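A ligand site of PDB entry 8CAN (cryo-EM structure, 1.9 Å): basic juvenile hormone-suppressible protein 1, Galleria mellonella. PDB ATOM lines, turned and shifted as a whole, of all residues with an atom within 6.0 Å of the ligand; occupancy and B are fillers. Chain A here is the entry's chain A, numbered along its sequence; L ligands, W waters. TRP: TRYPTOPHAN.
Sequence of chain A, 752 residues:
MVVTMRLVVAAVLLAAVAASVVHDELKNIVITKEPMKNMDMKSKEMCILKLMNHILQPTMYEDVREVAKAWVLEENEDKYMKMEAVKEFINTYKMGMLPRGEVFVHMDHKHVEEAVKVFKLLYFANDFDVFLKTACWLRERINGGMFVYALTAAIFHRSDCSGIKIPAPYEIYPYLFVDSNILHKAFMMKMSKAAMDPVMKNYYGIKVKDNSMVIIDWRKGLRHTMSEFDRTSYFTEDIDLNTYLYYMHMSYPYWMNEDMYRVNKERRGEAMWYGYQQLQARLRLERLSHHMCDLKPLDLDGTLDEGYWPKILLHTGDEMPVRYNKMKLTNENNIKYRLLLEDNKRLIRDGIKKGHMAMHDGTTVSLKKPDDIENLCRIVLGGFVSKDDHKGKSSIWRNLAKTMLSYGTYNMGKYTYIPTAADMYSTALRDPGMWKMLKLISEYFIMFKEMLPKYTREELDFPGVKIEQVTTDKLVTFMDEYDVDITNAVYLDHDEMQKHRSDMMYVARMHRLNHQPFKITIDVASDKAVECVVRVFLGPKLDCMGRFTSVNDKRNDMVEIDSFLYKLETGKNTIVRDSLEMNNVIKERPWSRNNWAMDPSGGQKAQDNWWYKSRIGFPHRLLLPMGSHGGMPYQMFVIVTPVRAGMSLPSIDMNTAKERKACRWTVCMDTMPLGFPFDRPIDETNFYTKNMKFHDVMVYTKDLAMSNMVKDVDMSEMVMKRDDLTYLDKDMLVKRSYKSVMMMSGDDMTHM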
ATOM      1  N   TYR A 244      -7.087   5.698 -33.655  1.00  0.00           N
ATOM      2  CA  TYR A 244      -6.794   4.730 -32.602  1.00  0.00           C
ATOM      3  C   TYR A 244      -5.324   4.337 -32.633  1.00  0.00           C
ATOM      4  O   TYR A 244      -4.676   4.257 -31.584  1.00  0.00           O
ATOM      5  CB  TYR A 244      -7.688   3.504 -32.769  1.00  0.00           C
ATOM      6  CG  TYR A 244      -7.447   2.418 -31.745  1.00  0.00           C
ATOM      7  CD1 TYR A 244      -8.049   2.471 -30.502  1.00  0.00           C
ATOM      8  CD2 TYR A 244      -6.642   1.331 -32.035  1.00  0.00           C
ATOM      9  CE1 TYR A 244      -7.838   1.478 -29.558  1.00  0.00           C
ATOM     10  CE2 TYR A 244      -6.425   0.329 -31.105  1.00  0.00           C
ATOM     11  CZ  TYR A 244      -7.030   0.413 -29.869  1.00  0.00           C
ATOM     12  OH  TYR A 244      -6.813  -0.579 -28.938  1.00  0.00           O
ATOM     13  N   TYR A 274      -0.573  -6.328 -28.084  1.00  0.00           N
ATOM     14  CA  TYR A 274      -1.929  -6.854 -28.136  1.00  0.00           C
ATOM     15  C   TYR A 274      -2.828  -5.959 -28.983  1.00  0.00           C
ATOM     16  O   TYR A 274      -3.730  -6.463 -29.657  1.00  0.00           O
ATOM     17  CB  TYR A 274      -2.503  -6.998 -26.730  1.00  0.00           C
ATOM     18  CG  TYR A 274      -3.735  -7.881 -26.652  1.00  0.00           C
ATOM     19  CD1 TYR A 274      -3.709  -9.171 -27.157  1.00  0.00           C
ATOM     20  CD2 TYR A 274      -4.899  -7.424 -26.070  1.00  0.00           C
ATOM     21  CE1 TYR A 274      -4.818  -9.984 -27.089  1.00  0.00           C
ATOM     22  CE2 TYR A 274      -6.026  -8.228 -25.994  1.00  0.00           C
ATOM     23  CZ  TYR A 274      -5.972  -9.508 -26.509  1.00  0.00           C
ATOM     24  OH  TYR A 274      -7.090 -10.321 -26.437  1.00  0.00           O
ATOM     25  N   GLY A 275      -2.589  -4.651 -28.978  1.00  0.00           N
ATOM     26  CA  GLY A 275      -3.328  -3.785 -29.884  1.00  0.00           C
ATOM     27  C   GLY A 275      -3.076  -4.126 -31.333  1.00  0.00           C
ATOM     28  O   GLY A 275      -4.017  -4.244 -32.136  1.00  0.00           O
ATOM     29  N   GLN A 278      -4.807  -7.512 -32.082  1.00  0.00           N
ATOM     30  CA  GLN A 278      -6.255  -7.383 -32.199  1.00  0.00           C
ATOM     31  C   GLN A 278      -6.642  -6.675 -33.485  1.00  0.00           C
ATOM     32  O   GLN A 278      -7.652  -7.020 -34.103  1.00  0.00           O
ATOM     33  CB  GLN A 278      -6.804  -6.639 -30.975  1.00  0.00           C
ATOM     34  CG  GLN A 278      -6.725  -7.435 -29.687  1.00  0.00           C
ATOM     35  CD  GLN A 278      -7.680  -8.618 -29.671  1.00  0.00           C
ATOM     36  OE1 GLN A 278      -8.886  -8.452 -29.533  1.00  0.00           O
ATOM     37  NE2 GLN A 278      -7.131  -9.818 -29.819  1.00  0.00           N
ATOM     38  N   LEU A 279      -5.873  -5.674 -33.901  1.00  0.00           N
ATOM     39  CA  LEU A 279      -6.144  -5.036 -35.190  1.00  0.00           C
ATOM     40  C   LEU A 279      -6.022  -6.040 -36.334  1.00  0.00           C
ATOM     41  O   LEU A 279      -6.863  -6.064 -37.244  1.00  0.00           O
ATOM     42  CB  LEU A 279      -5.188  -3.865 -35.410  1.00  0.00           C
ATOM     43  CG  LEU A 279      -5.407  -2.629 -34.528  1.00  0.00           C
ATOM     44  CD1 LEU A 279      -4.242  -1.663 -34.674  1.00  0.00           C
ATOM     45  CD2 LEU A 279      -6.721  -1.941 -34.882  1.00  0.00           C
ATOM     46  N   ARG A 282      -9.056  -8.317 -36.260  1.00  0.00           N
ATOM     47  CA  ARG A 282     -10.241  -7.625 -36.756  1.00  0.00           C
ATOM     48  C   ARG A 282     -10.218  -7.511 -38.272  1.00  0.00           C
ATOM     49  O   ARG A 282     -11.253  -7.714 -38.927  1.00  0.00           O
ATOM     50  CB  ARG A 282     -10.323  -6.240 -36.110  1.00  0.00           C
ATOM     51  CG  ARG A 282     -11.529  -5.411 -36.517  1.00  0.00           C
ATOM     52  CD  ARG A 282     -12.839  -6.057 -36.091  1.00  0.00           C
ATOM     53  NE  ARG A 282     -13.991  -5.250 -36.466  1.00  0.00           N
ATOM     54  CZ  ARG A 282     -14.527  -5.214 -37.675  1.00  0.00           C
ATOM     55  NH1 ARG A 282     -14.050  -5.958 -38.660  1.00  0.00           N
ATOM     56  NH2 ARG A 282     -15.561  -4.414 -37.902  1.00  0.00           N
ATOM     57  N   VAL A 559     -11.072 -11.927 -31.388  1.00  0.00           N
ATOM     58  CA  VAL A 559     -11.082 -10.522 -31.012  1.00  0.00           C
ATOM     59  C   VAL A 559     -11.788 -10.391 -29.673  1.00  0.00           C
ATOM     60  O   VAL A 559     -12.965 -10.766 -29.549  1.00  0.00           O
ATOM     61  CB  VAL A 559     -11.753  -9.650 -32.081  1.00  0.00           C
ATOM     62  CG1 VAL A 559     -11.745  -8.186 -31.655  1.00  0.00           C
ATOM     63  CG2 VAL A 559     -11.070  -9.820 -33.423  1.00  0.00           C
ATOM     64  N   GLU A 560     -11.086  -9.870 -28.669  1.00  0.00           N
ATOM     65  CA  GLU A 560     -11.643  -9.701 -27.330  1.00  0.00           C
ATOM     66  C   GLU A 560     -12.563  -8.490 -27.355  1.00  0.00           C
ATOM     67  O   GLU A 560     -12.150  -7.351 -27.166  1.00  0.00           O
ATOM     68  CB  GLU A 560     -10.525  -9.524 -26.301  1.00  0.00           C
ATOM     69  CG  GLU A 560     -11.001  -9.520 -24.860  1.00  0.00           C
ATOM     70  CD  GLU A 560      -9.853  -9.433 -23.868  1.00  0.00           C
ATOM     71  OE1 GLU A 560      -8.679  -9.515 -24.299  1.00  0.00           O
ATOM     72  OE2 GLU A 560     -10.126  -9.291 -22.655  1.00  0.00           O
ATOM     73  N   ILE A 561     -13.859  -8.748 -27.588  1.00  0.00           N
ATOM     74  CA  ILE A 561     -14.804  -7.652 -27.737  1.00  0.00           C
ATOM     75  C   ILE A 561     -15.275  -7.114 -26.391  1.00  0.00           C
ATOM     76  O   ILE A 561     -15.751  -5.971 -26.336  1.00  0.00           O
ATOM     77  CB  ILE A 561     -16.019  -8.076 -28.571  1.00  0.00           C
ATOM     78  CG1 ILE A 561     -16.758  -9.257 -27.930  1.00  0.00           C
ATOM     79  CG2 ILE A 561     -15.586  -8.421 -29.991  1.00  0.00           C
ATOM     80  CD1 ILE A 561     -18.058  -9.597 -28.612  1.00  0.00           C
ATOM     81  N   ASP A 562     -15.176  -7.881 -25.312  1.00  0.00           N
ATOM     82  CA  ASP A 562     -15.614  -7.371 -24.021  1.00  0.00           C
ATOM     83  C   ASP A 562     -14.839  -8.046 -22.896  1.00  0.00           C
ATOM     84  O   ASP A 562     -14.419  -9.196 -23.016  1.00  0.00           O
ATOM     85  CB  ASP A 562     -17.122  -7.576 -23.812  1.00  0.00           C
ATOM     86  CG  ASP A 562     -17.666  -6.800 -22.631  1.00  0.00           C
ATOM     87  OD1 ASP A 562     -16.886  -6.053 -21.997  1.00  0.00           O
ATOM     88  OD2 ASP A 562     -18.864  -6.932 -22.329  1.00  0.00           O
ATOM     89  N   SER A 563     -14.686  -7.323 -21.790  1.00  0.00           N
ATOM     90  CA  SER A 563     -14.044  -7.850 -20.588  1.00  0.00           C
ATOM     91  C   SER A 563     -14.483  -7.005 -19.410  1.00  0.00           C
ATOM     92  O   SER A 563     -14.405  -5.782 -19.468  1.00  0.00           O
ATOM     93  CB  SER A 563     -12.520  -7.839 -20.727  1.00  0.00           C
ATOM     94  OG  SER A 563     -12.040  -6.523 -20.938  1.00  0.00           O
ATOM     95  N   ASN A 583     -16.425  -2.484 -22.716  1.00  0.00           N
ATOM     96  CA  ASN A 583     -15.229  -1.805 -22.225  1.00  0.00           C
ATOM     97  C   ASN A 583     -14.495  -1.093 -23.355  1.00  0.00           C
ATOM     98  O   ASN A 583     -14.237  -1.672 -24.412  1.00  0.00           O
ATOM     99  CB  ASN A 583     -14.308  -2.813 -21.552  1.00  0.00           C
ATOM    100  CG  ASN A 583     -13.126  -2.152 -20.866  1.00  0.00           C
ATOM    101  OD1 ASN A 583     -13.209  -0.998 -20.431  1.00  0.00           O
ATOM    102  ND2 ASN A 583     -12.018  -2.877 -20.758  1.00  0.00           N
ATOM    103  N   ASN A 584     -14.145   0.174 -23.105  1.00  0.00           N
ATOM    104  CA  ASN A 584     -13.322   0.966 -24.018  1.00  0.00           C
ATOM    105  C   ASN A 584     -13.880   1.000 -25.433  1.00  0.00           C
ATOM    106  O   ASN A 584     -13.138   0.914 -26.409  1.00  0.00           O
ATOM    107  CB  ASN A 584     -11.875   0.452 -24.025  1.00  0.00           C
ATOM    108  CG  ASN A 584     -11.198   0.609 -22.688  1.00  0.00           C
ATOM    109  OD1 ASN A 584     -11.448   1.572 -21.956  1.00  0.00           O
ATOM    110  ND2 ASN A 584     -10.314  -0.334 -22.349  1.00  0.00           N
ATOM    111  N   VAL A 585     -15.201   1.118 -25.553  1.00  0.00           N
ATOM    112  CA  VAL A 585     -15.861   1.338 -26.837  1.00  0.00           C
ATOM    113  C   VAL A 585     -16.566   2.683 -26.764  1.00  0.00           C
ATOM    114  O   VAL A 585     -17.423   2.895 -25.900  1.00  0.00           O
ATOM    115  CB  VAL A 585     -16.847   0.200 -27.169  1.00  0.00           C
ATOM    116  CG1 VAL A 585     -17.235   0.256 -28.644  1.00  0.00           C
ATOM    117  CG2 VAL A 585     -16.244  -1.151 -26.821  1.00  0.00           C
ATOM    118  N   ILE A 616      -8.200   6.228 -25.323  1.00  0.00           N
ATOM    119  CA  ILE A 616      -7.946   4.799 -25.438  1.00  0.00           C
ATOM    120  C   ILE A 616      -9.162   4.041 -25.956  1.00  0.00           C
ATOM    121  O   ILE A 616      -9.250   2.825 -25.809  1.00  0.00           O
ATOM    122  CB  ILE A 616      -7.483   4.207 -24.088  1.00  0.00           C
ATOM    123  CG1 ILE A 616      -8.609   4.284 -23.058  1.00  0.00           C
ATOM    124  CG2 ILE A 616      -6.261   4.945 -23.584  1.00  0.00           C
ATOM    125  CD1 ILE A 616      -8.238   3.723 -21.695  1.00  0.00           C
ATOM    126  N   PHE A 618     -12.025   2.490 -28.649  1.00  0.00           N
ATOM    127  CA  PHE A 618     -12.215   1.897 -29.970  1.00  0.00           C
ATOM    128  C   PHE A 618     -13.593   2.262 -30.507  1.00  0.00           C
ATOM    129  O   PHE A 618     -14.580   2.200 -29.767  1.00  0.00           O
ATOM    130  CB  PHE A 618     -12.074   0.381 -29.899  1.00  0.00           C
ATOM    131  CG  PHE A 618     -12.018  -0.283 -31.249  1.00  0.00           C
ATOM    132  CD1 PHE A 618     -10.810  -0.437 -31.909  1.00  0.00           C
ATOM    133  CD2 PHE A 618     -13.167  -0.768 -31.843  1.00  0.00           C
ATOM    134  CE1 PHE A 618     -10.747  -1.046 -33.152  1.00  0.00           C
ATOM    135  CE2 PHE A 618     -13.114  -1.387 -33.084  1.00  0.00           C
ATOM    136  CZ  PHE A 618     -11.903  -1.521 -33.733  1.00  0.00           C
ATOM    137  N   LEU A 622     -17.128   0.249 -35.639  1.00  0.00           N
ATOM    138  CA  LEU A 622     -16.357  -0.899 -36.110  1.00  0.00           C
ATOM    139  C   LEU A 622     -16.383  -2.062 -35.120  1.00  0.00           C
ATOM    140  O   LEU A 622     -15.503  -2.928 -35.171  1.00  0.00           O
ATOM    141  CB  LEU A 622     -14.922  -0.470 -36.400  1.00  0.00           C
ATOM    142  CG  LEU A 622     -14.760   0.729 -37.341  1.00  0.00           C
ATOM    143  CD1 LEU A 622     -13.290   1.035 -37.564  1.00  0.00           C
ATOM    144  CD2 LEU A 622     -15.463   0.491 -38.662  1.00  0.00           C
ATOM    145  N   LEU A 623     -17.362  -2.091 -34.212  1.00  0.00           N
ATOM    146  CA  LEU A 623     -17.423  -3.163 -33.226  1.00  0.00           C
ATOM    147  C   LEU A 623     -17.629  -4.514 -33.905  1.00  0.00           C
ATOM    148  O   LEU A 623     -16.994  -5.506 -33.521  1.00  0.00           O
ATOM    149  CB  LEU A 623     -18.542  -2.884 -32.231  1.00  0.00           C
ATOM    150  CG  LEU A 623     -18.738  -3.930 -31.121  1.00  0.00           C
ATOM    151  CD1 LEU A 623     -17.476  -4.067 -30.287  1.00  0.00           C
ATOM    152  CD2 LEU A 623     -19.923  -3.555 -30.247  1.00  0.00           C
ATOM    153  N   CYS A 663      -6.521   2.181 -18.726  1.00  0.00           N
ATOM    154  CA  CYS A 663      -6.908   0.792 -18.467  1.00  0.00           C
ATOM    155  C   CYS A 663      -7.430   0.171 -19.765  1.00  0.00           C
ATOM    156  O   CYS A 663      -8.643   0.052 -20.000  1.00  0.00           O
ATOM    157  CB  CYS A 663      -7.942   0.725 -17.359  1.00  0.00           C
ATOM    158  SG  CYS A 663      -7.336   1.272 -15.744  1.00  0.00           S
ATOM    159  N   ARG A 664      -6.491  -0.242 -20.615  1.00  0.00           N
ATOM    160  CA  ARG A 664      -6.840  -0.979 -21.821  1.00  0.00           C
ATOM    161  C   ARG A 664      -6.989  -2.463 -21.494  1.00  0.00           C
ATOM    162  O   ARG A 664      -6.201  -3.032 -20.741  1.00  0.00           O
ATOM    163  CB  ARG A 664      -5.774  -0.793 -22.893  1.00  0.00           C
ATOM    164  CG  ARG A 664      -5.566   0.645 -23.351  1.00  0.00           C
ATOM    165  CD  ARG A 664      -4.438   0.738 -24.375  1.00  0.00           C
ATOM    166  NE  ARG A 664      -4.228   2.088 -24.858  1.00  0.00           N
ATOM    167  CZ  ARG A 664      -4.785   2.609 -25.942  1.00  0.00           C
ATOM    168  NH1 ARG A 664      -5.637   1.907 -26.686  1.00  0.00           N
ATOM    169  NH2 ARG A 664      -4.487   3.852 -26.302  1.00  0.00           N
ATOM    170  N   TRP A 665      -8.022  -3.080 -22.062  1.00  0.00           N
ATOM    171  CA  TRP A 665      -8.316  -4.506 -21.871  1.00  0.00           C
ATOM    172  C   TRP A 665      -8.426  -4.759 -20.362  1.00  0.00           C
ATOM    173  O   TRP A 665      -9.177  -4.040 -19.694  1.00  0.00           O
ATOM    174  CB  TRP A 665      -7.264  -5.337 -22.590  1.00  0.00           C
ATOM    175  CG  TRP A 665      -7.220  -5.114 -24.076  1.00  0.00           C
ATOM    176  CD1 TRP A 665      -8.125  -5.568 -24.992  1.00  0.00           C
ATOM    177  CD2 TRP A 665      -6.225  -4.412 -24.811  1.00  0.00           C
ATOM    178  NE1 TRP A 665      -7.755  -5.168 -26.248  1.00  0.00           N
ATOM    179  CE2 TRP A 665      -6.589  -4.462 -26.161  1.00  0.00           C
ATOM    180  CE3 TRP A 665      -5.046  -3.737 -24.453  1.00  0.00           C
ATOM    181  CZ2 TRP A 665      -5.830  -3.856 -27.166  1.00  0.00           C
ATOM    182  CZ3 TRP A 665      -4.293  -3.142 -25.445  1.00  0.00           C
ATOM    183  CH2 TRP A 665      -4.685  -3.202 -26.786  1.00  0.00           C
HETATM  184  N   TRP L   1     -11.660  -4.626 -26.123  1.00  0.00           N
HETATM  185  CA  TRP L   1     -10.751  -3.497 -26.296  1.00  0.00           C
HETATM  186  C   TRP L   1     -10.525  -2.784 -24.961  1.00  0.00           C
HETATM  187  O   TRP L   1      -9.619  -1.957 -24.827  1.00  0.00           O
HETATM  188  CB  TRP L   1     -11.303  -2.517 -27.329  1.00  0.00           C
HETATM  189  CG  TRP L   1     -11.493  -3.129 -28.683  1.00  0.00           C
HETATM  190  CD1 TRP L   1     -12.653  -3.647 -29.190  1.00  0.00           C
HETATM  191  CD2 TRP L   1     -10.497  -3.306 -29.692  1.00  0.00           C
HETATM  192  NE1 TRP L   1     -12.442  -4.126 -30.460  1.00  0.00           N
HETATM  193  CE2 TRP L   1     -11.127  -3.934 -30.791  1.00  0.00           C
HETATM  194  CE3 TRP L   1      -9.140  -2.994 -29.789  1.00  0.00           C
HETATM  195  CZ2 TRP L   1     -10.443  -4.252 -31.960  1.00  0.00           C
HETATM  196  CZ3 TRP L   1      -8.462  -3.312 -30.944  1.00  0.00           C
HETATM  197  CH2 TRP L   1      -9.117  -3.931 -32.023  1.00  0.00           C
HETATM  198  OXT TRP L   1     -11.244  -3.019 -23.986  1.00  0.00           O
HETATM  199  O   HOH W   1      -9.599  -6.323 -28.591  1.00  0.00           O
HETATM  200  O   HOH W   2     -14.118  -4.813 -33.034  1.00  0.00           O
HETATM  201  O   HOH W   3     -13.978  -4.042 -25.466  1.00  0.00           O
HETATM  202  O   HOH W   4     -11.666  -6.222 -23.648  1.00  0.00           O
HETATM  203  O   HOH W   5      -7.881  -0.036 -26.395  1.00  0.00           O
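O of Glu 560 lies within hydrogen-bond range of N of the ligand, at 3.0 Å. ND2 of Asn 584 lies within hydrogen-bond range of O of the ligand, at 3.0 Å. ND2 of Asn 583 is in hydrogen-bond range of OXT of the ligand. N of Trp 665 sits at hydrogen-bond distance from O of the ligand (3.4 Å).
The backbone NH of Glu 560 lies within hydrogen-bond range of the side-chain amide oxygen of Gln 278 (2.8 Å). The side-chain hydroxyl of Tyr 274 is in hydrogen-bond range of the side-chain carboxylate of Glu 560 (2.8 Å). The side-chain amide nitrogen (ND2) of Asn 584 sits close to the side-chain amide nitrogen (ND2) of Asn 583. N of Phe 618 is in hydrogen-bond range of O of Asn 584, at 3.0 Å. The side-chain amide nitrogen (ND2) of Asn 584 is in hydrogen-bond range of the backbone carbonyl oxygen (O) of Cys 663 (2.9 Å). ND2 of Asn 583 lies within hydrogen-bond range of O of Trp 665 (3.2 Å). The side-chain amide nitrogen (NE2) of Gln 278 is in hydrogen-bond range of the side-chain hydroxyl (OH) of Tyr 274 (3.4 Å).
Merely in contact with the ligand: Tyr 244 (3.5 Å), Gln 278 (3.7 Å) and Phe 618 (3.4 Å). Hydrophobic or aromatic side chains within 4 Å of the ligand: Phe 618 and Trp 665. Of the 21 residues printed, 7 come within 4 Å of the ligand. The nearest printed residue that does not touch the ligand is Leu 279 (4.1 Å).
Water W3 lies within hydrogen-bond range of a nitrogen (N) of the ligand, the backbone carbonyl oxygen of Asn 583 and the backbone carbonyl oxygen of Ile 561. Water W4 bridges the side-chain hydroxyl of Ser 563 (2.8 Å) and a nitrogen (N) of the ligand (2.9 Å). Water W5 lies within hydrogen-bond range of the side-chain hydroxyl (OH) of Tyr 244 (2.8 Å), the guanidinium group (NH1) of Arg 664 (3.0 Å), an oxygen (O) of the ligand (3.0 Å) and the backbone carbonyl oxygen (O) of Ile 616 (3.2 Å). Water W2 lies within hydrogen-bond range of the backbone carbonyl oxygen of Leu 623 (3.0 Å), a nitrogen (NE1) of the ligand (3.1 Å), the backbone carbonyl oxygen of Leu 622 (3.2 Å) and the guanidinium group of Arg 282 (3.5 Å). Water W1 lies within hydrogen-bond range of the side-chain amide oxygen (OE1) of Gln 278 (2.4 Å), the backbone carbonyl oxygen (O) of Glu 560 (3.1 Å) and the indole nitrogen (NE1) of Trp 665 (3.2 Å).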
